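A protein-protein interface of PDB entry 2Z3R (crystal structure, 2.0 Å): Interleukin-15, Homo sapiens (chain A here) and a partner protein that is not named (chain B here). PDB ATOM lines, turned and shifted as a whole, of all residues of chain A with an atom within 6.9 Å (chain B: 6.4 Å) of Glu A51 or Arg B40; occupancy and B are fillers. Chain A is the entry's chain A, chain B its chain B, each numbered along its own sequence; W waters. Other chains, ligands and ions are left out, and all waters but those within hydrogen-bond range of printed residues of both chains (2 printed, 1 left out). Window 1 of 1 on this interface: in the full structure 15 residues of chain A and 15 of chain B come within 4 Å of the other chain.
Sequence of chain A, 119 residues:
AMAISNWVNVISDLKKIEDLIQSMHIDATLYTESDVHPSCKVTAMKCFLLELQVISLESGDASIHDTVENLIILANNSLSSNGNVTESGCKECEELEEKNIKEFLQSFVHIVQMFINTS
OE1 of Glu A51 is in hydrogen-bond range of N of Tyr A31.
The side-chain sulfur (SG) of Cys A47 is disulfide-bonded to the side-chain sulfur (SG) of Cys A93, 2.0 Å away.
N of Lys B39 sits at hydrogen-bond distance from O of Ile B69 (2.7 Å).
The backbone carbonyl oxygen (O) of Thr B44 is in hydrogen-bond range of the guanidinium group (NH1) of Arg B40 (2.7 Å).
The backbone carbonyl oxygen (O) of Ser B45 sits at hydrogen-bond distance from the backbone NH (N) of Leu B66, 2.9 Å away.
SG of Cys B34 is disulfide-bonded to SG of Cys B68.
Water W2 bridges OE1 of Glu A98 (2.4 Å) and NE of Arg B40 (2.8 Å).
Water W1 bridges the side-chain carboxylate (OE2) of Glu A58 (2.8 Å) and the backbone NH (N) of Ser B46 (3.0 Å).
Lys B39 touches Tyr A31 (CB to OH, 3.8 Å).
Tyr A31 touches Ala B42.
Leu A50 touches Gly B43.
OE2 of Glu A51 touches CA of Ala B42, 3.6 Å away.
C of Gly B43 touches CG2 of Val A54 (3.5 Å).
CB of Ala B42 touches CB of Cys A93, 3.5 Å away.
CB of Lys B39 touches CB of Glu A94, 3.9 Å away.
CG of Glu A94 touches O of Arg B40 (3.2 Å).
Glu A94 touches Lys B41 (OE2 to CA, 3.6 Å).
Ile B69 touches Glu A94 (CD1 to CD, 3.6 Å).
The guanidinium group of Arg B40 is in hydrogen-bond range of the backbone carbonyl oxygen of Thr A29 (3.3 Å).
OH of Tyr A31 sits at hydrogen-bond distance from O of Arg B40, at 2.6 Å.
The guanidinium group (NH2) of Arg B40 lies within salt-bridge range of the side-chain carboxylate (OE1) of Glu A51 (3.0 Å).
The side-chain carboxylate of Glu A51 sits at hydrogen-bond distance from the backbone NH of Gly B43 (2.8 Å).
The side-chain carboxylate of Glu A58 sits at hydrogen-bond distance from the side-chain hydroxyl of Ser B45.
OE2 of Glu A94 is in hydrogen-bond range of N of Ala B42.
The side-chain carboxylate of Glu A98 is in salt-bridge range of the guanidinium group of Arg B40, 3.8 Å away.
Of the printed residues of chain B, Glu A51 touches Arg B40, Ala B42 and Gly B43.
Arg B40 touches five residues of chain A.
Printed residues of chain B within 4 Å of Val A54: Gly B43 (3.5 Å) and Thr B44 (3.4 Å).
Of the printed residues of chain B, Cys A93 touches Ala B42.
Of the printed residues of chain A, Thr B44 touches Val A54 (3.4 Å).
Ile A101 touches none of the printed residues of chain B.
Leu B66 touches none of the printed residues of chain A.
The nearest printed residue of chain B that does not touch Glu A51 is Thr B44 (4.7 Å).
The nearest residue of chain A that does not touch Arg B40 is Val A54 (4.1 Å).
The nearest printed residue of chain B that does not touch Cys A93 is Arg B40 (6.5 Å).
Among the printed residues, 19 pairs touch across the chains.
Among the printed residues, Asp or Glu carboxylates within 4 Å of a Lys or Arg side-chain nitrogen of the other chain: Glu A51 with Arg B40 and Glu A98 with Arg B40.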
ATOM      1  N   ALA A  28       5.757   8.856 -22.687  1.00  0.00           N
ATOM      2  CA  ALA A  28       6.689   7.821 -22.291  1.00  0.00           C
ATOM      3  C   ALA A  28       6.346   6.532 -23.026  1.00  0.00           C
ATOM      4  O   ALA A  28       5.180   6.297 -23.363  1.00  0.00           O
ATOM      5  CB  ALA A  28       6.625   7.594 -20.819  1.00  0.00           C
ATOM      6  N   THR A  29       7.377   5.738 -23.288  1.00  0.00           N
ATOM      7  CA  THR A  29       7.213   4.377 -23.741  1.00  0.00           C
ATOM      8  C   THR A  29       7.574   3.479 -22.570  1.00  0.00           C
ATOM      9  O   THR A  29       8.471   3.790 -21.766  1.00  0.00           O
ATOM     10  CB  THR A  29       8.016   4.096 -25.027  1.00  0.00           C
ATOM     11  OG1 THR A  29       9.426   4.206 -24.789  1.00  0.00           O
ATOM     12  CG2 THR A  29       7.642   5.104 -26.105  1.00  0.00           C
ATOM     13  N   LEU A  30       6.839   2.395 -22.426  1.00  0.00           N
ATOM     14  CA  LEU A  30       6.891   1.607 -21.213  1.00  0.00           C
ATOM     15  C   LEU A  30       7.008   0.117 -21.528  1.00  0.00           C
ATOM     16  O   LEU A  30       6.403  -0.364 -22.486  1.00  0.00           O
ATOM     17  CB  LEU A  30       5.617   1.856 -20.414  1.00  0.00           C
ATOM     18  CG  LEU A  30       5.322   3.292 -20.014  1.00  0.00           C
ATOM     19  CD1 LEU A  30       3.909   3.363 -19.598  1.00  0.00           C
ATOM     20  CD2 LEU A  30       6.278   3.752 -18.878  1.00  0.00           C
ATOM     21  N   TYR A  31       7.770  -0.612 -20.708  1.00  0.00           N
ATOM     22  CA  TYR A  31       7.910  -2.047 -20.886  1.00  0.00           C
ATOM     23  C   TYR A  31       6.549  -2.724 -20.773  1.00  0.00           C
ATOM     24  O   TYR A  31       5.795  -2.503 -19.826  1.00  0.00           O
ATOM     25  CB  TYR A  31       8.866  -2.593 -19.869  1.00  0.00           C
ATOM     26  CG  TYR A  31      10.252  -1.963 -19.922  1.00  0.00           C
ATOM     27  CD1 TYR A  31      10.998  -1.991 -21.080  1.00  0.00           C
ATOM     28  CD2 TYR A  31      10.816  -1.373 -18.790  1.00  0.00           C
ATOM     29  CE1 TYR A  31      12.275  -1.440 -21.137  1.00  0.00           C
ATOM     30  CE2 TYR A  31      12.112  -0.837 -18.824  1.00  0.00           C
ATOM     31  CZ  TYR A  31      12.823  -0.871 -20.006  1.00  0.00           C
ATOM     32  OH  TYR A  31      14.108  -0.371 -20.066  1.00  0.00           O
ATOM     33  N   THR A  32       6.220  -3.527 -21.776  1.00  0.00           N
ATOM     34  CA  THR A  32       4.853  -3.993 -21.919  1.00  0.00           C
ATOM     35  C   THR A  32       4.880  -5.434 -22.371  1.00  0.00           C
ATOM     36  O   THR A  32       5.319  -5.702 -23.462  1.00  0.00           O
ATOM     37  CB  THR A  32       4.029  -3.133 -22.944  1.00  0.00           C
ATOM     38  OG1 THR A  32       3.963  -1.754 -22.512  1.00  0.00           O
ATOM     39  CG2 THR A  32       2.601  -3.691 -23.074  1.00  0.00           C
ATOM     40  N   LYS A  46       4.215  -7.463 -11.747  1.00  0.00           N
ATOM     41  CA  LYS A  46       5.127  -6.557 -11.092  1.00  0.00           C
ATOM     42  C   LYS A  46       5.745  -5.515 -12.060  1.00  0.00           C
ATOM     43  O   LYS A  46       5.950  -4.370 -11.672  1.00  0.00           O
ATOM     44  CB  LYS A  46       6.167  -7.365 -10.262  1.00  0.00           C
ATOM     45  CG  LYS A  46       5.498  -8.043  -9.024  1.00  0.00           C
ATOM     46  CD  LYS A  46       6.512  -8.646  -8.016  1.00  0.00           C
ATOM     47  CE  LYS A  46       5.808  -9.075  -6.705  1.00  0.00           C
ATOM     48  NZ  LYS A  46       6.792  -9.622  -5.669  1.00  0.00           N
ATOM     49  N   CYS A  47       5.991  -5.878 -13.323  1.00  0.00           N
ATOM     50  CA  CYS A  47       6.532  -4.911 -14.275  1.00  0.00           C
ATOM     51  C   CYS A  47       5.537  -3.857 -14.606  1.00  0.00           C
ATOM     52  O   CYS A  47       5.864  -2.691 -14.615  1.00  0.00           O
ATOM     53  CB  CYS A  47       7.007  -5.572 -15.560  1.00  0.00           C
ATOM     54  SG  CYS A  47       8.391  -6.719 -15.282  1.00  0.00           S
ATOM     55  N   PHE A  48       4.296  -4.286 -14.849  1.00  0.00           N
ATOM     56  CA  PHE A  48       3.187  -3.368 -15.131  1.00  0.00           C
ATOM     57  C   PHE A  48       3.023  -2.330 -13.992  1.00  0.00           C
ATOM     58  O   PHE A  48       2.827  -1.126 -14.206  1.00  0.00           O
ATOM     59  CB  PHE A  48       1.898  -4.164 -15.349  1.00  0.00           C
ATOM     60  CG  PHE A  48       1.709  -4.664 -16.793  1.00  0.00           C
ATOM     61  CD1 PHE A  48       1.336  -3.787 -17.817  1.00  0.00           C
ATOM     62  CD2 PHE A  48       1.856  -6.006 -17.107  1.00  0.00           C
ATOM     63  CE1 PHE A  48       1.138  -4.230 -19.129  1.00  0.00           C
ATOM     64  CE2 PHE A  48       1.655  -6.470 -18.419  1.00  0.00           C
ATOM     65  CZ  PHE A  48       1.289  -5.572 -19.427  1.00  0.00           C
ATOM     66  N   LEU A  49       3.112  -2.823 -12.779  1.00  0.00           N
ATOM     67  CA  LEU A  49       2.957  -1.972 -11.629  1.00  0.00           C
ATOM     68  C   LEU A  49       4.077  -0.977 -11.520  1.00  0.00           C
ATOM     69  O   LEU A  49       3.851   0.178 -11.187  1.00  0.00           O
ATOM     70  CB  LEU A  49       2.870  -2.810 -10.340  1.00  0.00           C
ATOM     71  CG  LEU A  49       1.674  -3.751 -10.262  1.00  0.00           C
ATOM     72  CD1 LEU A  49       1.853  -4.771  -9.107  1.00  0.00           C
ATOM     73  CD2 LEU A  49       0.365  -2.982 -10.110  1.00  0.00           C
ATOM     74  N   LEU A  50       5.293  -1.426 -11.746  1.00  0.00           N
ATOM     75  CA  LEU A  50       6.460  -0.496 -11.718  1.00  0.00           C
ATOM     76  C   LEU A  50       6.342   0.606 -12.782  1.00  0.00           C
ATOM     77  O   LEU A  50       6.632   1.779 -12.504  1.00  0.00           O
ATOM     78  CB  LEU A  50       7.756  -1.276 -11.915  1.00  0.00           C
ATOM     79  CG  LEU A  50       8.358  -2.027 -10.719  1.00  0.00           C
ATOM     80  CD1 LEU A  50       9.493  -2.900 -11.156  1.00  0.00           C
ATOM     81  CD2 LEU A  50       8.869  -1.063  -9.651  1.00  0.00           C
ATOM     82  N   GLU A  51       5.881   0.228 -13.982  1.00  0.00           N
ATOM     83  CA  GLU A  51       5.829   1.144 -15.112  1.00  0.00           C
ATOM     84  C   GLU A  51       4.628   2.066 -14.993  1.00  0.00           C
ATOM     85  O   GLU A  51       4.668   3.167 -15.486  1.00  0.00           O
ATOM     86  CB  GLU A  51       5.772   0.387 -16.439  1.00  0.00           C
ATOM     87  CG  GLU A  51       7.072  -0.323 -16.845  1.00  0.00           C
ATOM     88  CD  GLU A  51       8.152   0.661 -17.294  1.00  0.00           C
ATOM     89  OE1 GLU A  51       8.330   0.802 -18.512  1.00  0.00           O
ATOM     90  OE2 GLU A  51       8.811   1.297 -16.446  1.00  0.00           O
ATOM     91  N   LEU A  52       3.578   1.639 -14.298  1.00  0.00           N
ATOM     92  CA  LEU A  52       2.483   2.574 -14.023  1.00  0.00           C
ATOM     93  C   LEU A  52       2.991   3.762 -13.219  1.00  0.00           C
ATOM     94  O   LEU A  52       2.493   4.854 -13.346  1.00  0.00           O
ATOM     95  CB  LEU A  52       1.386   1.879 -13.251  1.00  0.00           C
ATOM     96  CG  LEU A  52       0.092   2.668 -13.046  1.00  0.00           C
ATOM     97  CD1 LEU A  52      -0.576   3.035 -14.370  1.00  0.00           C
ATOM     98  CD2 LEU A  52      -0.791   1.822 -12.140  1.00  0.00           C
ATOM     99  N   GLN A  53       3.989   3.529 -12.394  1.00  0.00           N
ATOM    100  CA  GLN A  53       4.539   4.595 -11.551  1.00  0.00           C
ATOM    101  C   GLN A  53       5.253   5.696 -12.332  1.00  0.00           C
ATOM    102  O   GLN A  53       5.363   6.828 -11.859  1.00  0.00           O
ATOM    103  CB  GLN A  53       5.504   4.015 -10.569  1.00  0.00           C
ATOM    104  CG  GLN A  53       4.899   3.012  -9.515  1.00  0.00           C
ATOM    105  CD  GLN A  53       5.910   2.704  -8.393  1.00  0.00           C
ATOM    106  OE1 GLN A  53       5.845   3.281  -7.314  1.00  0.00           O
ATOM    107  NE2 GLN A  53       6.865   1.815  -8.663  1.00  0.00           N
ATOM    108  N   VAL A  54       5.794   5.332 -13.501  1.00  0.00           N
ATOM    109  CA  VAL A  54       6.397   6.258 -14.402  1.00  0.00           C
ATOM    110  C   VAL A  54       5.315   7.185 -14.963  1.00  0.00           C
ATOM    111  O   VAL A  54       5.532   8.379 -15.077  1.00  0.00           O
ATOM    112  CB  VAL A  54       7.075   5.451 -15.525  1.00  0.00           C
ATOM    113  CG1 VAL A  54       7.480   6.369 -16.709  1.00  0.00           C
ATOM    114  CG2 VAL A  54       8.308   4.740 -14.927  1.00  0.00           C
ATOM    115  N   ILE A  55       4.157   6.618 -15.334  1.00  0.00           N
ATOM    116  CA  ILE A  55       2.985   7.421 -15.846  1.00  0.00           C
ATOM    117  C   ILE A  55       2.571   8.399 -14.768  1.00  0.00           C
ATOM    118  O   ILE A  55       2.483   9.587 -14.973  1.00  0.00           O
ATOM    119  CB  ILE A  55       1.766   6.547 -16.247  1.00  0.00           C
ATOM    120  CG1 ILE A  55       2.072   5.710 -17.497  1.00  0.00           C
ATOM    121  CG2 ILE A  55       0.495   7.432 -16.465  1.00  0.00           C
ATOM    122  CD1 ILE A  55       1.040   4.501 -17.796  1.00  0.00           C
ATOM    123  N   SER A  56       2.403   7.892 -13.577  1.00  0.00           N
ATOM    124  CA  SER A  56       2.156   8.750 -12.423  1.00  0.00           C
ATOM    125  C   SER A  56       3.188   9.870 -12.205  1.00  0.00           C
ATOM    126  O   SER A  56       2.813  11.045 -12.147  1.00  0.00           O
ATOM    127  CB  SER A  56       2.017   7.870 -11.219  1.00  0.00           C
ATOM    128  OG  SER A  56       1.817   8.657 -10.101  1.00  0.00           O
ATOM    129  N   GLU A  58       5.572  11.133 -14.263  1.00  0.00           N
ATOM    130  CA  GLU A  58       5.609  12.019 -15.401  1.00  0.00           C
ATOM    131  C   GLU A  58       4.349  12.891 -15.538  1.00  0.00           C
ATOM    132  O   GLU A  58       4.407  13.990 -16.090  1.00  0.00           O
ATOM    133  CB  GLU A  58       5.970  11.228 -16.646  1.00  0.00           C
ATOM    134  CG  GLU A  58       7.406  10.614 -16.505  1.00  0.00           C
ATOM    135  CD  GLU A  58       7.967  10.142 -17.811  1.00  0.00           C
ATOM    136  OE1 GLU A  58       7.309  10.357 -18.842  1.00  0.00           O
ATOM    137  OE2 GLU A  58       9.066   9.560 -17.822  1.00  0.00           O
ATOM    138  N   CYS A  93      11.969  -7.194 -16.496  1.00  0.00           N
ATOM    139  CA  CYS A  93      11.104  -6.138 -17.092  1.00  0.00           C
ATOM    140  C   CYS A  93      11.765  -5.446 -18.285  1.00  0.00           C
ATOM    141  O   CYS A  93      11.111  -5.152 -19.273  1.00  0.00           O
ATOM    142  CB  CYS A  93      10.748  -5.049 -16.091  1.00  0.00           C
ATOM    143  SG  CYS A  93       9.965  -5.628 -14.624  1.00  0.00           S
ATOM    144  N   GLU A  94      13.064  -5.201 -18.170  1.00  0.00           N
ATOM    145  CA  GLU A  94      13.815  -4.505 -19.228  1.00  0.00           C
ATOM    146  C   GLU A  94      14.057  -5.334 -20.503  1.00  0.00           C
ATOM    147  O   GLU A  94      14.575  -4.824 -21.496  1.00  0.00           O
ATOM    148  CB  GLU A  94      15.130  -3.944 -18.677  1.00  0.00           C
ATOM    149  CG  GLU A  94      14.931  -2.953 -17.522  1.00  0.00           C
ATOM    150  CD  GLU A  94      14.594  -3.642 -16.188  1.00  0.00           C
ATOM    151  OE1 GLU A  94      14.746  -4.885 -16.079  1.00  0.00           O
ATOM    152  OE2 GLU A  94      14.175  -2.918 -15.261  1.00  0.00           O
ATOM    153  N   GLU A  98       8.968  -2.043 -25.634  1.00  0.00           N
ATOM    154  CA  GLU A  98       8.411  -0.817 -25.117  1.00  0.00           C
ATOM    155  C   GLU A  98       7.305  -0.317 -26.015  1.00  0.00           C
ATOM    156  O   GLU A  98       7.455  -0.256 -27.239  1.00  0.00           O
ATOM    157  CB  GLU A  98       9.496   0.251 -24.997  1.00  0.00           C
ATOM    158  CG  GLU A  98      10.525  -0.074 -23.933  1.00  0.00           C
ATOM    159  CD  GLU A  98      11.576   0.984 -23.857  1.00  0.00           C
ATOM    160  OE1 GLU A  98      11.271   2.086 -23.341  1.00  0.00           O
ATOM    161  OE2 GLU A  98      12.703   0.717 -24.333  1.00  0.00           O
ATOM    162  N   ILE A 101       1.622   4.556 -24.203  1.00  0.00           N
ATOM    163  CA  ILE A 101       0.761   4.458 -23.048  1.00  0.00           C
ATOM    164  C   ILE A 101      -0.552   3.751 -23.307  1.00  0.00           C
ATOM    165  O   ILE A 101      -1.045   3.030 -22.462  1.00  0.00           O
ATOM    166  CB  ILE A 101       0.421   5.838 -22.513  1.00  0.00           C
ATOM    167  CG1 ILE A 101       1.698   6.634 -22.287  1.00  0.00           C
ATOM    168  CG2 ILE A 101      -0.347   5.712 -21.199  1.00  0.00           C
ATOM    169  CD1 ILE A 101       2.192   6.679 -20.801  1.00  0.00           C
ATOM    170  N   PHE A 104       0.154   0.068 -23.603  1.00  0.00           N
ATOM    171  CA  PHE A 104       0.516  -0.292 -22.258  1.00  0.00           C
ATOM    172  C   PHE A 104      -0.762  -0.572 -21.426  1.00  0.00           C
ATOM    173  O   PHE A 104      -0.962  -1.695 -20.963  1.00  0.00           O
ATOM    174  CB  PHE A 104       1.372   0.795 -21.625  1.00  0.00           C
ATOM    175  CG  PHE A 104       1.733   0.494 -20.197  1.00  0.00           C
ATOM    176  CD1 PHE A 104       2.747  -0.395 -19.907  1.00  0.00           C
ATOM    177  CD2 PHE A 104       1.018   1.067 -19.148  1.00  0.00           C
ATOM    178  CE1 PHE A 104       3.068  -0.707 -18.614  1.00  0.00           C
ATOM    179  CE2 PHE A 104       1.341   0.755 -17.819  1.00  0.00           C
ATOM    180  CZ  PHE A 104       2.368  -0.148 -17.560  1.00  0.00           C
ATOM    181  N   PHE A 108      -2.296  -3.957 -19.754  1.00  0.00           N
ATOM    182  CA  PHE A 108      -2.456  -3.977 -18.295  1.00  0.00           C
ATOM    183  C   PHE A 108      -3.860  -4.535 -17.966  1.00  0.00           C
ATOM    184  O   PHE A 108      -4.034  -5.455 -17.132  1.00  0.00           O
ATOM    185  CB  PHE A 108      -2.206  -2.554 -17.713  1.00  0.00           C
ATOM    186  CG  PHE A 108      -1.754  -2.511 -16.241  1.00  0.00           C
ATOM    187  CD1 PHE A 108      -1.029  -1.431 -15.770  1.00  0.00           C
ATOM    188  CD2 PHE A 108      -2.098  -3.519 -15.342  1.00  0.00           C
ATOM    189  CE1 PHE A 108      -0.647  -1.335 -14.428  1.00  0.00           C
ATOM    190  CE2 PHE A 108      -1.684  -3.444 -14.000  1.00  0.00           C
ATOM    191  CZ  PHE A 108      -0.979  -2.354 -13.547  1.00  0.00           C
ATOM    192  N   CYS B  34      19.498   5.847 -22.274  1.00  0.00           N
ATOM    193  CA  CYS B  34      20.553   4.974 -21.753  1.00  0.00           C
ATOM    194  C   CYS B  34      21.429   4.599 -22.913  1.00  0.00           C
ATOM    195  O   CYS B  34      20.937   4.463 -24.025  1.00  0.00           O
ATOM    196  CB  CYS B  34      19.968   3.741 -21.119  1.00  0.00           C
ATOM    197  SG  CYS B  34      19.063   4.091 -19.582  1.00  0.00           S
ATOM    198  N   PHE B  38      22.902  -0.625 -22.126  1.00  0.00           N
ATOM    199  CA  PHE B  38      22.226  -0.342 -20.844  1.00  0.00           C
ATOM    200  C   PHE B  38      20.748  -0.184 -21.140  1.00  0.00           C
ATOM    201  O   PHE B  38      20.431   0.153 -22.246  1.00  0.00           O
ATOM    202  CB  PHE B  38      22.748   0.940 -20.207  1.00  0.00           C
ATOM    203  CG  PHE B  38      24.101   0.790 -19.597  1.00  0.00           C
ATOM    204  CD1 PHE B  38      24.236   0.462 -18.238  1.00  0.00           C
ATOM    205  CD2 PHE B  38      25.220   0.957 -20.383  1.00  0.00           C
ATOM    206  CE1 PHE B  38      25.483   0.343 -17.685  1.00  0.00           C
ATOM    207  CE2 PHE B  38      26.507   0.817 -19.812  1.00  0.00           C
ATOM    208  CZ  PHE B  38      26.617   0.496 -18.482  1.00  0.00           C
ATOM    209  N   LYS B  39      19.881  -0.353 -20.151  1.00  0.00           N
ATOM    210  CA  LYS B  39      18.428  -0.175 -20.325  1.00  0.00           C
ATOM    211  C   LYS B  39      17.875   0.656 -19.170  1.00  0.00           C
ATOM    212  O   LYS B  39      18.395   0.585 -18.053  1.00  0.00           O
ATOM    213  CB  LYS B  39      17.719  -1.524 -20.354  1.00  0.00           C
ATOM    214  CG  LYS B  39      18.037  -2.368 -21.581  1.00  0.00           C
ATOM    215  CD  LYS B  39      17.111  -1.976 -22.719  1.00  0.00           C
ATOM    216  CE  LYS B  39      17.580  -2.543 -24.047  1.00  0.00           C
ATOM    217  NZ  LYS B  39      16.840  -1.840 -25.162  1.00  0.00           N
ATOM    218  N   ARG B  40      16.829   1.443 -19.415  1.00  0.00           N
ATOM    219  CA  ARG B  40      16.174   2.186 -18.350  1.00  0.00           C
ATOM    220  C   ARG B  40      15.573   1.196 -17.336  1.00  0.00           C
ATOM    221  O   ARG B  40      14.894   0.259 -17.716  1.00  0.00           O
ATOM    222  CB  ARG B  40      15.095   3.089 -18.925  1.00  0.00           C
ATOM    223  CG  ARG B  40      14.319   3.891 -17.859  1.00  0.00           C
ATOM    224  CD  ARG B  40      13.148   4.676 -18.444  1.00  0.00           C
ATOM    225  NE  ARG B  40      12.288   3.838 -19.263  1.00  0.00           N
ATOM    226  CZ  ARG B  40      11.289   3.104 -18.784  1.00  0.00           C
ATOM    227  NH1 ARG B  40      11.001   3.098 -17.475  1.00  0.00           N
ATOM    228  NH2 ARG B  40      10.581   2.380 -19.616  1.00  0.00           N
ATOM    229  N   LYS B  41      15.876   1.370 -16.057  1.00  0.00           N
ATOM    230  CA  LYS B  41      15.299   0.522 -15.027  1.00  0.00           C
ATOM    231  C   LYS B  41      13.763   0.688 -14.949  1.00  0.00           C
ATOM    232  O   LYS B  41      13.245   1.796 -14.837  1.00  0.00           O
ATOM    233  CB  LYS B  41      15.962   0.778 -13.663  1.00  0.00           C
ATOM    234  CG  LYS B  41      15.627  -0.314 -12.681  1.00  0.00           C
ATOM    235  CD  LYS B  41      16.054   0.052 -11.325  1.00  0.00           C
ATOM    236  CE  LYS B  41      15.813  -1.070 -10.358  1.00  0.00           C
ATOM    237  NZ  LYS B  41      16.226  -0.611  -8.995  1.00  0.00           N
ATOM    238  N   ALA B  42      13.028  -0.424 -15.019  1.00  0.00           N
ATOM    239  CA  ALA B  42      11.595  -0.361 -14.939  1.00  0.00           C
ATOM    240  C   ALA B  42      11.151   0.462 -13.749  1.00  0.00           C
ATOM    241  O   ALA B  42      11.654   0.299 -12.629  1.00  0.00           O
ATOM    242  CB  ALA B  42      10.979  -1.787 -14.915  1.00  0.00           C
ATOM    243  N   GLY B  43      10.193   1.347 -13.963  1.00  0.00           N
ATOM    244  CA  GLY B  43       9.727   2.158 -12.845  1.00  0.00           C
ATOM    245  C   GLY B  43      10.546   3.400 -12.569  1.00  0.00           C
ATOM    246  O   GLY B  43      10.227   4.149 -11.635  1.00  0.00           O
ATOM    247  N   THR B  44      11.617   3.605 -13.347  1.00  0.00           N
ATOM    248  CA  THR B  44      12.336   4.884 -13.372  1.00  0.00           C
ATOM    249  C   THR B  44      11.992   5.631 -14.655  1.00  0.00           C
ATOM    250  O   THR B  44      11.647   4.994 -15.643  1.00  0.00           O
ATOM    251  CB  THR B  44      13.877   4.767 -13.126  1.00  0.00           C
ATOM    252  OG1 THR B  44      14.552   4.267 -14.289  1.00  0.00           O
ATOM    253  CG2 THR B  44      14.149   3.899 -11.955  1.00  0.00           C
ATOM    254  N   SER B  45      12.010   6.975 -14.586  1.00  0.00           N
ATOM    255  CA  SER B  45      11.604   7.880 -15.668  1.00  0.00           C
ATOM    256  C   SER B  45      12.808   8.615 -16.282  1.00  0.00           C
ATOM    257  O   SER B  45      13.682   9.037 -15.572  1.00  0.00           O
ATOM    258  CB  SER B  45      10.649   8.924 -15.088  1.00  0.00           C
ATOM    259  OG  SER B  45      10.566  10.081 -15.929  1.00  0.00           O
ATOM    260  N   SER B  46      12.856   8.743 -17.614  1.00  0.00           N
ATOM    261  CA  SER B  46      13.963   9.463 -18.281  1.00  0.00           C
ATOM    262  C   SER B  46      13.649  10.969 -18.474  1.00  0.00           C
ATOM    263  O   SER B  46      14.443  11.685 -19.064  1.00  0.00           O
ATOM    264  CB  SER B  46      14.252   8.846 -19.662  1.00  0.00           C
ATOM    265  OG  SER B  46      13.036   8.542 -20.321  1.00  0.00           O
ATOM    266  N   LEU B  66      15.609   8.334 -13.572  1.00  0.00           N
ATOM    267  CA  LEU B  66      16.230   7.328 -14.444  1.00  0.00           C
ATOM    268  C   LEU B  66      17.391   6.613 -13.782  1.00  0.00           C
ATOM    269  O   LEU B  66      18.237   7.216 -13.134  1.00  0.00           O
ATOM    270  CB  LEU B  66      16.735   7.957 -15.745  1.00  0.00           C
ATOM    271  CG  LEU B  66      17.486   7.097 -16.759  1.00  0.00           C
ATOM    272  CD1 LEU B  66      16.672   5.897 -17.218  1.00  0.00           C
ATOM    273  CD2 LEU B  66      17.830   7.962 -17.918  1.00  0.00           C
ATOM    274  N   LYS B  67      17.439   5.308 -13.951  1.00  0.00           N
ATOM    275  CA  LYS B  67      18.632   4.603 -13.586  1.00  0.00           C
ATOM    276  C   LYS B  67      18.905   3.666 -14.734  1.00  0.00           C
ATOM    277  O   LYS B  67      18.019   2.916 -15.178  1.00  0.00           O
ATOM    278  CB  LYS B  67      18.412   3.886 -12.242  1.00  0.00           C
ATOM    279  CG  LYS B  67      19.431   2.846 -11.862  1.00  0.00           C
ATOM    280  CD  LYS B  67      20.840   3.389 -11.820  1.00  0.00           C
ATOM    281  CE  LYS B  67      21.809   2.318 -11.329  1.00  0.00           C
ATOM    282  NZ  LYS B  67      22.081   2.552  -9.894  1.00  0.00           N
ATOM    283  N   CYS B  68      20.123   3.708 -15.244  1.00  0.00           N
ATOM    284  CA  CYS B  68      20.436   2.861 -16.397  1.00  0.00           C
ATOM    285  C   CYS B  68      21.107   1.599 -15.923  1.00  0.00           C
ATOM    286  O   CYS B  68      22.136   1.654 -15.259  1.00  0.00           O
ATOM    287  CB  CYS B  68      21.303   3.589 -17.423  1.00  0.00           C
ATOM    288  SG  CYS B  68      20.443   4.908 -18.280  1.00  0.00           S
ATOM    289  N   ILE B  69      20.538   0.450 -16.249  1.00  0.00           N
ATOM    290  CA  ILE B  69      21.115  -0.801 -15.741  1.00  0.00           C
ATOM    291  C   ILE B  69      21.654  -1.575 -16.893  1.00  0.00           C
ATOM    292  O   ILE B  69      21.140  -1.464 -17.993  1.00  0.00           O
ATOM    293  CB  ILE B  69      20.094  -1.706 -14.977  1.00  0.00           C
ATOM    294  CG1 ILE B  69      18.900  -2.098 -15.859  1.00  0.00           C
ATOM    295  CG2 ILE B  69      19.632  -1.048 -13.708  1.00  0.00           C
ATOM    296  CD1 ILE B  69      18.063  -3.221 -15.214  1.00  0.00           C
HETATM  297  O   HOH W   1      10.447   7.343 -18.771  1.00  0.00           O
HETATM  298  O   HOH W   2      12.203   3.885 -22.044  1.00  0.00           O
